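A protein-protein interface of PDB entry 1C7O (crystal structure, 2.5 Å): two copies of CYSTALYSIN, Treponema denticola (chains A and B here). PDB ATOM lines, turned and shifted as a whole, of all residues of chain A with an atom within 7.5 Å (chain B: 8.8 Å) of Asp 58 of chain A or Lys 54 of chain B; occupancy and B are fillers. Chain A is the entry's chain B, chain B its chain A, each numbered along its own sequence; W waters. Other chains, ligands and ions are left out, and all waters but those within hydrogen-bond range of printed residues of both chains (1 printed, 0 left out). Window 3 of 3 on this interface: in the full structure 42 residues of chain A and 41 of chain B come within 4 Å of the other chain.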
ATOM      1  N   ILE A  50     -14.862  -0.198 -15.474  1.00  0.00           N
ATOM      2  CA  ILE A  50     -13.853   0.849 -15.502  1.00  0.00           C
ATOM      3  C   ILE A  50     -12.471   0.356 -15.050  1.00  0.00           C
ATOM      4  O   ILE A  50     -11.481   0.514 -15.774  1.00  0.00           O
ATOM      5  CB  ILE A  50     -14.302   2.046 -14.636  1.00  0.00           C
ATOM      6  CG1 ILE A  50     -15.654   2.567 -15.145  1.00  0.00           C
ATOM      7  CG2 ILE A  50     -13.261   3.138 -14.665  1.00  0.00           C
ATOM      8  CD1 ILE A  50     -15.666   2.896 -16.609  1.00  0.00           C
ATOM      9  N   GLY A  52     -11.354  -2.614 -14.905  1.00  0.00           N
ATOM     10  CA  GLY A  52     -10.894  -3.610 -15.860  1.00  0.00           C
ATOM     11  C   GLY A  52     -10.322  -3.080 -17.158  1.00  0.00           C
ATOM     12  O   GLY A  52      -9.340  -3.615 -17.678  1.00  0.00           O
ATOM     13  N   LEU A  53     -10.942  -2.040 -17.700  1.00  0.00           N
ATOM     14  CA  LEU A  53     -10.466  -1.455 -18.939  1.00  0.00           C
ATOM     15  C   LEU A  53      -9.142  -0.739 -18.691  1.00  0.00           C
ATOM     16  O   LEU A  53      -8.234  -0.804 -19.520  1.00  0.00           O
ATOM     17  CB  LEU A  53     -11.507  -0.482 -19.485  1.00  0.00           C
ATOM     18  CG  LEU A  53     -12.838  -1.129 -19.873  1.00  0.00           C
ATOM     19  CD1 LEU A  53     -13.915  -0.056 -20.030  1.00  0.00           C
ATOM     20  CD2 LEU A  53     -12.656  -1.922 -21.151  1.00  0.00           C
ATOM     21  N   LYS A  54      -9.028  -0.059 -17.552  1.00  0.00           N
ATOM     22  CA  LYS A  54      -7.793   0.648 -17.225  1.00  0.00           C
ATOM     23  C   LYS A  54      -6.659  -0.360 -17.088  1.00  0.00           C
ATOM     24  O   LYS A  54      -5.580  -0.179 -17.647  1.00  0.00           O
ATOM     25  CB  LYS A  54      -7.952   1.443 -15.921  1.00  0.00           C
ATOM     26  CG  LYS A  54      -9.035   2.513 -15.985  1.00  0.00           C
ATOM     27  CD  LYS A  54      -8.874   3.570 -14.901  1.00  0.00           C
ATOM     28  CE  LYS A  54      -9.121   3.010 -13.517  1.00  0.00           C
ATOM     29  NZ  LYS A  54      -9.096   4.082 -12.480  1.00  0.00           N
ATOM     30  N   LYS A  55      -6.922  -1.433 -16.351  1.00  0.00           N
ATOM     31  CA  LYS A  55      -5.941  -2.490 -16.131  1.00  0.00           C
ATOM     32  C   LYS A  55      -5.552  -3.101 -17.463  1.00  0.00           C
ATOM     33  O   LYS A  55      -4.398  -3.462 -17.677  1.00  0.00           O
ATOM     34  CB  LYS A  55      -6.541  -3.557 -15.221  1.00  0.00           C
ATOM     35  CG  LYS A  55      -5.668  -4.769 -14.963  1.00  0.00           C
ATOM     36  CD  LYS A  55      -6.371  -5.700 -13.974  1.00  0.00           C
ATOM     37  CE  LYS A  55      -5.592  -6.977 -13.739  1.00  0.00           C
ATOM     38  NZ  LYS A  55      -5.412  -7.747 -15.000  1.00  0.00           N
ATOM     39  N   TYR A  56      -6.526  -3.195 -18.362  1.00  0.00           N
ATOM     40  CA  TYR A  56      -6.308  -3.763 -19.683  1.00  0.00           C
ATOM     41  C   TYR A  56      -5.385  -2.892 -20.535  1.00  0.00           C
ATOM     42  O   TYR A  56      -4.528  -3.407 -21.258  1.00  0.00           O
ATOM     43  CB  TYR A  56      -7.648  -3.945 -20.395  1.00  0.00           C
ATOM     44  CG  TYR A  56      -7.565  -4.775 -21.655  1.00  0.00           C
ATOM     45  CD1 TYR A  56      -7.844  -4.222 -22.900  1.00  0.00           C
ATOM     46  CD2 TYR A  56      -7.224  -6.119 -21.600  1.00  0.00           C
ATOM     47  CE1 TYR A  56      -7.788  -4.988 -24.062  1.00  0.00           C
ATOM     48  CE2 TYR A  56      -7.162  -6.894 -22.754  1.00  0.00           C
ATOM     49  CZ  TYR A  56      -7.446  -6.322 -23.982  1.00  0.00           C
ATOM     50  OH  TYR A  56      -7.379  -7.082 -25.127  1.00  0.00           O
ATOM     51  N   LEU A  57      -5.559  -1.578 -20.449  1.00  0.00           N
ATOM     52  CA  LEU A  57      -4.742  -0.650 -21.221  1.00  0.00           C
ATOM     53  C   LEU A  57      -3.251  -0.821 -20.963  1.00  0.00           C
ATOM     54  O   LEU A  57      -2.433  -0.534 -21.837  1.00  0.00           O
ATOM     55  CB  LEU A  57      -5.157   0.790 -20.927  1.00  0.00           C
ATOM     56  CG  LEU A  57      -6.442   1.231 -21.619  1.00  0.00           C
ATOM     57  CD1 LEU A  57      -6.925   2.546 -21.038  1.00  0.00           C
ATOM     58  CD2 LEU A  57      -6.184   1.356 -23.112  1.00  0.00           C
ATOM     59  N   ASP A  58      -2.902  -1.292 -19.769  1.00  0.00           N
ATOM     60  CA  ASP A  58      -1.500  -1.501 -19.414  1.00  0.00           C
ATOM     61  C   ASP A  58      -0.972  -2.861 -19.842  1.00  0.00           C
ATOM     62  O   ASP A  58       0.191  -3.169 -19.598  1.00  0.00           O
ATOM     63  CB  ASP A  58      -1.290  -1.372 -17.901  1.00  0.00           C
ATOM     64  CG  ASP A  58      -1.427   0.045 -17.416  1.00  0.00           C
ATOM     65  OD1 ASP A  58      -0.832   0.945 -18.046  1.00  0.00           O
ATOM     66  OD2 ASP A  58      -2.124   0.259 -16.400  1.00  0.00           O
ATOM     67  N   GLU A  59      -1.808  -3.671 -20.479  1.00  0.00           N
ATOM     68  CA  GLU A  59      -1.387  -5.009 -20.883  1.00  0.00           C
ATOM     69  C   GLU A  59      -1.524  -5.281 -22.374  1.00  0.00           C
ATOM     70  O   GLU A  59      -1.123  -6.346 -22.853  1.00  0.00           O
ATOM     71  CB  GLU A  59      -2.211  -6.063 -20.141  1.00  0.00           C
ATOM     72  CG  GLU A  59      -2.654  -5.657 -18.751  1.00  0.00           C
ATOM     73  CD  GLU A  59      -3.596  -6.668 -18.136  1.00  0.00           C
ATOM     74  OE1 GLU A  59      -4.545  -7.096 -18.833  1.00  0.00           O
ATOM     75  OE2 GLU A  59      -3.393  -7.029 -16.956  1.00  0.00           O
ATOM     76  N   THR A  60      -2.083  -4.336 -23.116  1.00  0.00           N
ATOM     77  CA  THR A  60      -2.282  -4.567 -24.536  1.00  0.00           C
ATOM     78  C   THR A  60      -2.027  -3.358 -25.429  1.00  0.00           C
ATOM     79  O   THR A  60      -2.018  -2.214 -24.975  1.00  0.00           O
ATOM     80  CB  THR A  60      -3.729  -5.088 -24.789  1.00  0.00           C
ATOM     81  OG1 THR A  60      -3.851  -5.556 -26.139  1.00  0.00           O
ATOM     82  CG2 THR A  60      -4.740  -3.974 -24.545  1.00  0.00           C
ATOM     83  N   VAL A  61      -1.829  -3.643 -26.709  1.00  0.00           N
ATOM     84  CA  VAL A  61      -1.594  -2.628 -27.722  1.00  0.00           C
ATOM     85  C   VAL A  61      -2.911  -2.399 -28.461  1.00  0.00           C
ATOM     86  O   VAL A  61      -3.640  -3.347 -28.740  1.00  0.00           O
ATOM     87  CB  VAL A  61      -0.503  -3.098 -28.698  1.00  0.00           C
ATOM     88  CG1 VAL A  61      -0.340  -2.104 -29.825  1.00  0.00           C
ATOM     89  CG2 VAL A  61       0.810  -3.265 -27.947  1.00  0.00           C
ATOM     90  N   LYS B  44       4.628  -0.219 -28.030  1.00  0.00           N
ATOM     91  CA  LYS B  44       3.592   0.103 -27.064  1.00  0.00           C
ATOM     92  C   LYS B  44       3.039   1.457 -27.478  1.00  0.00           C
ATOM     93  O   LYS B  44       3.759   2.274 -28.055  1.00  0.00           O
ATOM     94  CB  LYS B  44       4.171   0.171 -25.651  1.00  0.00           C
ATOM     95  CG  LYS B  44       4.021  -1.127 -24.837  1.00  0.00           C
ATOM     96  CD  LYS B  44       2.540  -1.417 -24.507  1.00  0.00           C
ATOM     97  CE  LYS B  44       2.343  -2.613 -23.560  1.00  0.00           C
ATOM     98  NZ  LYS B  44       2.746  -3.914 -24.160  1.00  0.00           N
ATOM     99  N   ASN B  45       1.761   1.687 -27.205  1.00  0.00           N
ATOM    100  CA  ASN B  45       1.119   2.951 -27.556  1.00  0.00           C
ATOM    101  C   ASN B  45       1.719   4.137 -26.811  1.00  0.00           C
ATOM    102  O   ASN B  45       2.277   3.984 -25.724  1.00  0.00           O
ATOM    103  CB  ASN B  45      -0.377   2.866 -27.258  1.00  0.00           C
ATOM    104  CG  ASN B  45      -1.103   1.973 -28.226  1.00  0.00           C
ATOM    105  OD1 ASN B  45      -1.274   2.320 -29.399  1.00  0.00           O
ATOM    106  ND2 ASN B  45      -1.523   0.805 -27.756  1.00  0.00           N
ATOM    107  N   PRO B  47       2.625   6.911 -24.344  1.00  0.00           N
ATOM    108  CA  PRO B  47       2.291   6.987 -22.926  1.00  0.00           C
ATOM    109  C   PRO B  47       1.187   7.992 -22.649  1.00  0.00           C
ATOM    110  O   PRO B  47       0.253   7.700 -21.905  1.00  0.00           O
ATOM    111  CB  PRO B  47       3.612   7.398 -22.282  1.00  0.00           C
ATOM    112  CG  PRO B  47       4.627   6.822 -23.207  1.00  0.00           C
ATOM    113  CD  PRO B  47       4.059   7.177 -24.552  1.00  0.00           C
ATOM    114  N   GLU B  48       1.292   9.171 -23.251  1.00  0.00           N
ATOM    115  CA  GLU B  48       0.295  10.222 -23.039  1.00  0.00           C
ATOM    116  C   GLU B  48      -1.110   9.723 -23.345  1.00  0.00           C
ATOM    117  O   GLU B  48      -2.064  10.048 -22.635  1.00  0.00           O
ATOM    118  CB  GLU B  48       0.602  11.458 -23.902  1.00  0.00           C
ATOM    119  CG  GLU B  48       1.915  12.160 -23.558  1.00  0.00           C
ATOM    120  CD  GLU B  48       3.132  11.549 -24.252  1.00  0.00           C
ATOM    121  OE1 GLU B  48       4.274  11.867 -23.845  1.00  0.00           O
ATOM    122  OE2 GLU B  48       2.949  10.768 -25.211  1.00  0.00           O
ATOM    123  N   LEU B  49      -1.227   8.931 -24.403  1.00  0.00           N
ATOM    124  CA  LEU B  49      -2.510   8.376 -24.809  1.00  0.00           C
ATOM    125  C   LEU B  49      -3.071   7.486 -23.720  1.00  0.00           C
ATOM    126  O   LEU B  49      -4.217   7.644 -23.302  1.00  0.00           O
ATOM    127  CB  LEU B  49      -2.359   7.544 -26.086  1.00  0.00           C
ATOM    128  CG  LEU B  49      -3.649   6.861 -26.554  1.00  0.00           C
ATOM    129  CD1 LEU B  49      -4.689   7.922 -26.879  1.00  0.00           C
ATOM    130  CD2 LEU B  49      -3.375   6.002 -27.771  1.00  0.00           C
ATOM    131  N   ILE B  50      -2.247   6.543 -23.274  1.00  0.00           N
ATOM    132  CA  ILE B  50      -2.645   5.596 -22.249  1.00  0.00           C
ATOM    133  C   ILE B  50      -3.081   6.294 -20.968  1.00  0.00           C
ATOM    134  O   ILE B  50      -4.180   6.056 -20.465  1.00  0.00           O
ATOM    135  CB  ILE B  50      -1.493   4.604 -21.935  1.00  0.00           C
ATOM    136  CG1 ILE B  50      -1.124   3.819 -23.200  1.00  0.00           C
ATOM    137  CG2 ILE B  50      -1.900   3.650 -20.817  1.00  0.00           C
ATOM    138  CD1 ILE B  50      -2.297   3.116 -23.868  1.00  0.00           C
ATOM    139  N   GLU B  51      -2.229   7.165 -20.442  1.00  0.00           N
ATOM    140  CA  GLU B  51      -2.567   7.860 -19.213  1.00  0.00           C
ATOM    141  C   GLU B  51      -3.825   8.686 -19.409  1.00  0.00           C
ATOM    142  O   GLU B  51      -4.674   8.770 -18.517  1.00  0.00           O
ATOM    143  CB  GLU B  51      -1.421   8.770 -18.770  1.00  0.00           C
ATOM    144  CG  GLU B  51      -0.048   8.102 -18.692  1.00  0.00           C
ATOM    145  CD  GLU B  51      -0.107   6.589 -18.486  1.00  0.00           C
ATOM    146  OE1 GLU B  51      -0.815   6.125 -17.558  1.00  0.00           O
ATOM    147  OE2 GLU B  51       0.574   5.869 -19.259  1.00  0.00           O
ATOM    148  N   GLY B  52      -3.935   9.303 -20.579  1.00  0.00           N
ATOM    149  CA  GLY B  52      -5.097  10.118 -20.880  1.00  0.00           C
ATOM    150  C   GLY B  52      -6.361   9.280 -20.888  1.00  0.00           C
ATOM    151  O   GLY B  52      -7.349   9.637 -20.248  1.00  0.00           O
ATOM    152  N   LEU B  53      -6.325   8.156 -21.597  1.00  0.00           N
ATOM    153  CA  LEU B  53      -7.481   7.276 -21.679  1.00  0.00           C
ATOM    154  C   LEU B  53      -7.963   6.781 -20.320  1.00  0.00           C
ATOM    155  O   LEU B  53      -9.148   6.758 -20.060  1.00  0.00           O
ATOM    156  CB  LEU B  53      -7.174   6.078 -22.582  1.00  0.00           C
ATOM    157  CG  LEU B  53      -6.961   6.396 -24.062  1.00  0.00           C
ATOM    158  CD1 LEU B  53      -6.566   5.122 -24.818  1.00  0.00           C
ATOM    159  CD2 LEU B  53      -8.229   6.994 -24.641  1.00  0.00           C
ATOM    160  N   LYS B  54      -7.040   6.386 -19.457  1.00  0.00           N
ATOM    161  CA  LYS B  54      -7.393   5.885 -18.138  1.00  0.00           C
ATOM    162  C   LYS B  54      -8.065   6.955 -17.286  1.00  0.00           C
ATOM    163  O   LYS B  54      -8.997   6.670 -16.527  1.00  0.00           O
ATOM    164  CB  LYS B  54      -6.140   5.366 -17.425  1.00  0.00           C
ATOM    165  CG  LYS B  54      -5.354   4.382 -18.256  1.00  0.00           C
ATOM    166  CD  LYS B  54      -4.491   3.453 -17.418  1.00  0.00           C
ATOM    167  CE  LYS B  54      -3.138   4.044 -17.095  1.00  0.00           C
ATOM    168  NZ  LYS B  54      -2.233   3.000 -16.534  1.00  0.00           N
ATOM    169  N   LYS B  55      -7.577   8.186 -17.424  1.00  0.00           N
ATOM    170  CA  LYS B  55      -8.091   9.344 -16.694  1.00  0.00           C
ATOM    171  C   LYS B  55      -9.509   9.660 -17.167  1.00  0.00           C
ATOM    172  O   LYS B  55     -10.399   9.980 -16.380  1.00  0.00           O
ATOM    173  CB  LYS B  55      -7.167  10.545 -16.945  1.00  0.00           C
ATOM    174  CG  LYS B  55      -7.665  11.901 -16.450  1.00  0.00           C
ATOM    175  CD  LYS B  55      -6.687  13.014 -16.864  1.00  0.00           C
ATOM    176  CE  LYS B  55      -6.959  14.344 -16.153  1.00  0.00           C
ATOM    177  NZ  LYS B  55      -8.232  14.997 -16.566  1.00  0.00           N
ATOM    178  N   TYR B  56      -9.705   9.558 -18.471  1.00  0.00           N
ATOM    179  CA  TYR B  56     -10.995   9.832 -19.064  1.00  0.00           C
ATOM    180  C   TYR B  56     -12.017   8.782 -18.623  1.00  0.00           C
ATOM    181  O   TYR B  56     -13.206   9.075 -18.465  1.00  0.00           O
ATOM    182  CB  TYR B  56     -10.855   9.839 -20.588  1.00  0.00           C
ATOM    183  CG  TYR B  56     -12.082  10.313 -21.317  1.00  0.00           C
ATOM    184  CD1 TYR B  56     -12.795   9.456 -22.157  1.00  0.00           C
ATOM    185  CD2 TYR B  56     -12.537  11.620 -21.162  1.00  0.00           C
ATOM    186  CE1 TYR B  56     -13.934   9.895 -22.829  1.00  0.00           C
ATOM    187  CE2 TYR B  56     -13.672  12.068 -21.826  1.00  0.00           C
ATOM    188  CZ  TYR B  56     -14.367  11.202 -22.657  1.00  0.00           C
ATOM    189  OH  TYR B  56     -15.494  11.656 -23.300  1.00  0.00           O
ATOM    190  N   LEU B  57     -11.547   7.558 -18.415  1.00  0.00           N
ATOM    191  CA  LEU B  57     -12.428   6.478 -18.007  1.00  0.00           C
ATOM    192  C   LEU B  57     -13.021   6.690 -16.618  1.00  0.00           C
ATOM    193  O   LEU B  57     -14.114   6.204 -16.331  1.00  0.00           O
ATOM    194  CB  LEU B  57     -11.686   5.136 -18.075  1.00  0.00           C
ATOM    195  CG  LEU B  57     -11.439   4.595 -19.490  1.00  0.00           C
ATOM    196  CD1 LEU B  57     -10.527   3.379 -19.439  1.00  0.00           C
ATOM    197  CD2 LEU B  57     -12.770   4.234 -20.141  1.00  0.00           C
ATOM    198  N   ASP B  58     -12.314   7.417 -15.759  1.00  0.00           N
ATOM    199  CA  ASP B  58     -12.816   7.666 -14.414  1.00  0.00           C
ATOM    200  C   ASP B  58     -13.777   8.844 -14.434  1.00  0.00           C
ATOM    201  O   ASP B  58     -14.558   9.036 -13.499  1.00  0.00           O
ATOM    202  CB  ASP B  58     -11.666   7.952 -13.431  1.00  0.00           C
ATOM    203  CG  ASP B  58     -10.794   6.723 -13.149  1.00  0.00           C
ATOM    204  OD1 ASP B  58     -11.336   5.647 -12.795  1.00  0.00           O
ATOM    205  OD2 ASP B  58      -9.554   6.839 -13.272  1.00  0.00           O
ATOM    206  N   GLU B  59     -13.734   9.619 -15.511  1.00  0.00           N
ATOM    207  CA  GLU B  59     -14.590  10.798 -15.639  1.00  0.00           C
ATOM    208  C   GLU B  59     -15.899  10.593 -16.403  1.00  0.00           C
ATOM    209  O   GLU B  59     -16.958  11.054 -15.977  1.00  0.00           O
ATOM    210  CB  GLU B  59     -13.841  11.939 -16.353  1.00  0.00           C
ATOM    211  CG  GLU B  59     -12.484  12.329 -15.777  1.00  0.00           C
ATOM    212  CD  GLU B  59     -11.802  13.449 -16.577  1.00  0.00           C
ATOM    213  OE1 GLU B  59     -11.610  13.296 -17.810  1.00  0.00           O
ATOM    214  OE2 GLU B  59     -11.452  14.482 -15.968  1.00  0.00           O
ATOM    215  N   THR B  60     -15.813   9.893 -17.528  1.00  0.00           N
ATOM    216  CA  THR B  60     -16.949   9.728 -18.426  1.00  0.00           C
ATOM    217  C   THR B  60     -18.001   8.643 -18.207  1.00  0.00           C
ATOM    218  O   THR B  60     -17.946   7.863 -17.261  1.00  0.00           O
ATOM    219  CB  THR B  60     -16.422   9.620 -19.895  1.00  0.00           C
ATOM    220  OG1 THR B  60     -17.463   9.969 -20.813  1.00  0.00           O
ATOM    221  CG2 THR B  60     -15.932   8.202 -20.198  1.00  0.00           C
ATOM    222  N   MET B 245      -8.879   1.660 -32.181  1.00  0.00           N
ATOM    223  CA  MET B 245      -9.719   2.667 -31.527  1.00  0.00           C
ATOM    224  C   MET B 245     -10.842   3.117 -32.460  1.00  0.00           C
ATOM    225  O   MET B 245     -11.737   3.879 -32.074  1.00  0.00           O
ATOM    226  CB  MET B 245      -8.885   3.865 -31.074  1.00  0.00           C
ATOM    227  CG  MET B 245      -8.085   3.586 -29.803  1.00  0.00           C
ATOM    228  SD  MET B 245      -9.107   3.221 -28.334  1.00  0.00           S
ATOM    229  CE  MET B 245      -8.867   4.660 -27.355  1.00  0.00           C
ATOM    230  N   LEU B 276     -14.396   6.464 -26.784  1.00  0.00           N
ATOM    231  CA  LEU B 276     -12.938   6.505 -26.645  1.00  0.00           C
ATOM    232  C   LEU B 276     -12.239   6.814 -27.965  1.00  0.00           C
ATOM    233  O   LEU B 276     -11.161   7.431 -27.982  1.00  0.00           O
ATOM    234  CB  LEU B 276     -12.409   5.185 -26.075  1.00  0.00           C
ATOM    235  CG  LEU B 276     -12.949   4.800 -24.692  1.00  0.00           C
ATOM    236  CD1 LEU B 276     -12.359   3.465 -24.282  1.00  0.00           C
ATOM    237  CD2 LEU B 276     -12.605   5.865 -23.674  1.00  0.00           C
ATOM    238  N   LYS B 279     -11.752  10.508 -28.218  1.00  0.00           N
ATOM    239  CA  LYS B 279     -10.768  10.965 -27.245  1.00  0.00           C
ATOM    240  C   LYS B 279      -9.324  10.596 -27.616  1.00  0.00           C
ATOM    241  O   LYS B 279      -8.407  11.404 -27.456  1.00  0.00           O
ATOM    242  CB  LYS B 279     -11.108  10.398 -25.865  1.00  0.00           C
ATOM    243  CG  LYS B 279     -10.325  11.023 -24.736  1.00  0.00           C
ATOM    244  CD  LYS B 279     -10.614  12.515 -24.666  1.00  0.00           C
ATOM    245  CE  LYS B 279     -10.000  13.157 -23.432  1.00  0.00           C
ATOM    246  NZ  LYS B 279     -10.315  14.613 -23.389  1.00  0.00           N
ATOM    247  N   ILE B 283      -6.294  13.294 -28.091  1.00  0.00           N
ATOM    248  CA  ILE B 283      -5.067  13.238 -27.295  1.00  0.00           C
ATOM    249  C   ILE B 283      -3.780  13.041 -28.120  1.00  0.00           C
ATOM    250  O   ILE B 283      -2.813  13.792 -27.952  1.00  0.00           O
ATOM    251  CB  ILE B 283      -5.134  12.125 -26.241  1.00  0.00           C
ATOM    252  CG1 ILE B 283      -6.406  12.271 -25.403  1.00  0.00           C
ATOM    253  CG2 ILE B 283      -3.910  12.206 -25.330  1.00  0.00           C
ATOM    254  CD1 ILE B 283      -6.521  11.241 -24.310  1.00  0.00           C
HETATM  255  O   HOH W   1      -0.034   0.298 -25.373  1.00  0.00           O
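The side-chain amino group (NZ) of Lys 54 of chain B lies within salt-bridge range of the side-chain carboxylate (OD2) of Asp 58 of chain A (2.7 Å).
NZ of Lys 54 of chain A lies within salt-bridge range of OD1 of Asp 58 of chain B (2.8 Å).
NZ of Lys 54 of chain B lies within salt-bridge range of OE1 of Glu 51 of chain B (3.6 Å).
Among the printed residues, pairs that only touch across the chains: Ile 50 of chain A with Leu 57 of chain B (3.6 Å), Ile 50 of chain A with Asp 58 of chain B (3.7 Å), Leu 53 of chain A with Leu 57 of chain B (3.98 Å), Lys 54 of chain A with Lys 54 of chain B (3.5 Å), Lys 54 of chain A with Leu 57 of chain B (3.9 Å), Leu 57 of chain A with Leu 53 of chain B (3.9 Å), Leu 57 of chain A with Lys 54 of chain B (3.7 Å) and Val 61 of chain A with Asn 45 of chain B (3.4 Å).
Printed residues of chain B within 4 Å of Ile 50 of chain A: Leu 57 (3.6 Å) and Asp 58 (3.7 Å).
Printed residues of chain B within 4 Å of Lys 54 of chain A: Lys 54, Leu 57 and Asp 58.
Of the printed residues of chain B, Asp 58 of chain A touches Lys 54 (2.7 Å).
Of the printed residues of chain B, Val 61 of chain A touches Asn 45.
Lys 54 of chain B touches three residues of chain A.
Lys 55 of chain B touches none of the printed residues of chain A.
Printed residues of chain A within 4 Å of Leu 57 of chain B: Ile 50 (3.6 Å), Leu 53 (3.98 Å) and Lys 54 (3.9 Å).
The nearest printed residue of chain B that does not touch Asp 58 of chain A is Ile 50 of chain B (4.02 Å).
The nearest printed residue of chain B that does not touch Val 61 of chain A is Lys 44 of chain B (4.3 Å).
Of the 11 printed residues of chain A, 6 touch a printed residue of chain B.
Hydrophobic or aromatic side chains of chain A within 4 Å of the printed part of chain B: Ile 50, Leu 53, Leu 57 and Val 61.
Of the 20 printed residues of chain B, 5 touch a printed residue of chain A.
Ile 50 of chain A touches Asp 58 of chain B, but with the chains exchanged Asp 58 of chain A does not touch Ile 50 of chain B (4.02 Å).
Leu 53 of chain A touches Leu 57 of chain B, and with the chains exchanged Leu 57 of chain A touches Leu 53 of chain B.
Lys 54 of chain B touches its own counterpart, Lys 54 of chain A.
Lys 54 of chain A touches Leu 57 of chain B, and with the chains exchanged Leu 57 of chain A touches Lys 54 of chain B.
Positions printed for both chains: 50, 52, 53, 54, 55, 56, 57, 58, 59 and 60.
Of the 10 pairs that touch across the chains among the printed residues, 7 have their exchanged pair printed and touching as well.
Water W1 lies within hydrogen-bond range of ND2 of Asn 45 of chain B and O of Thr 60 of chain A.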
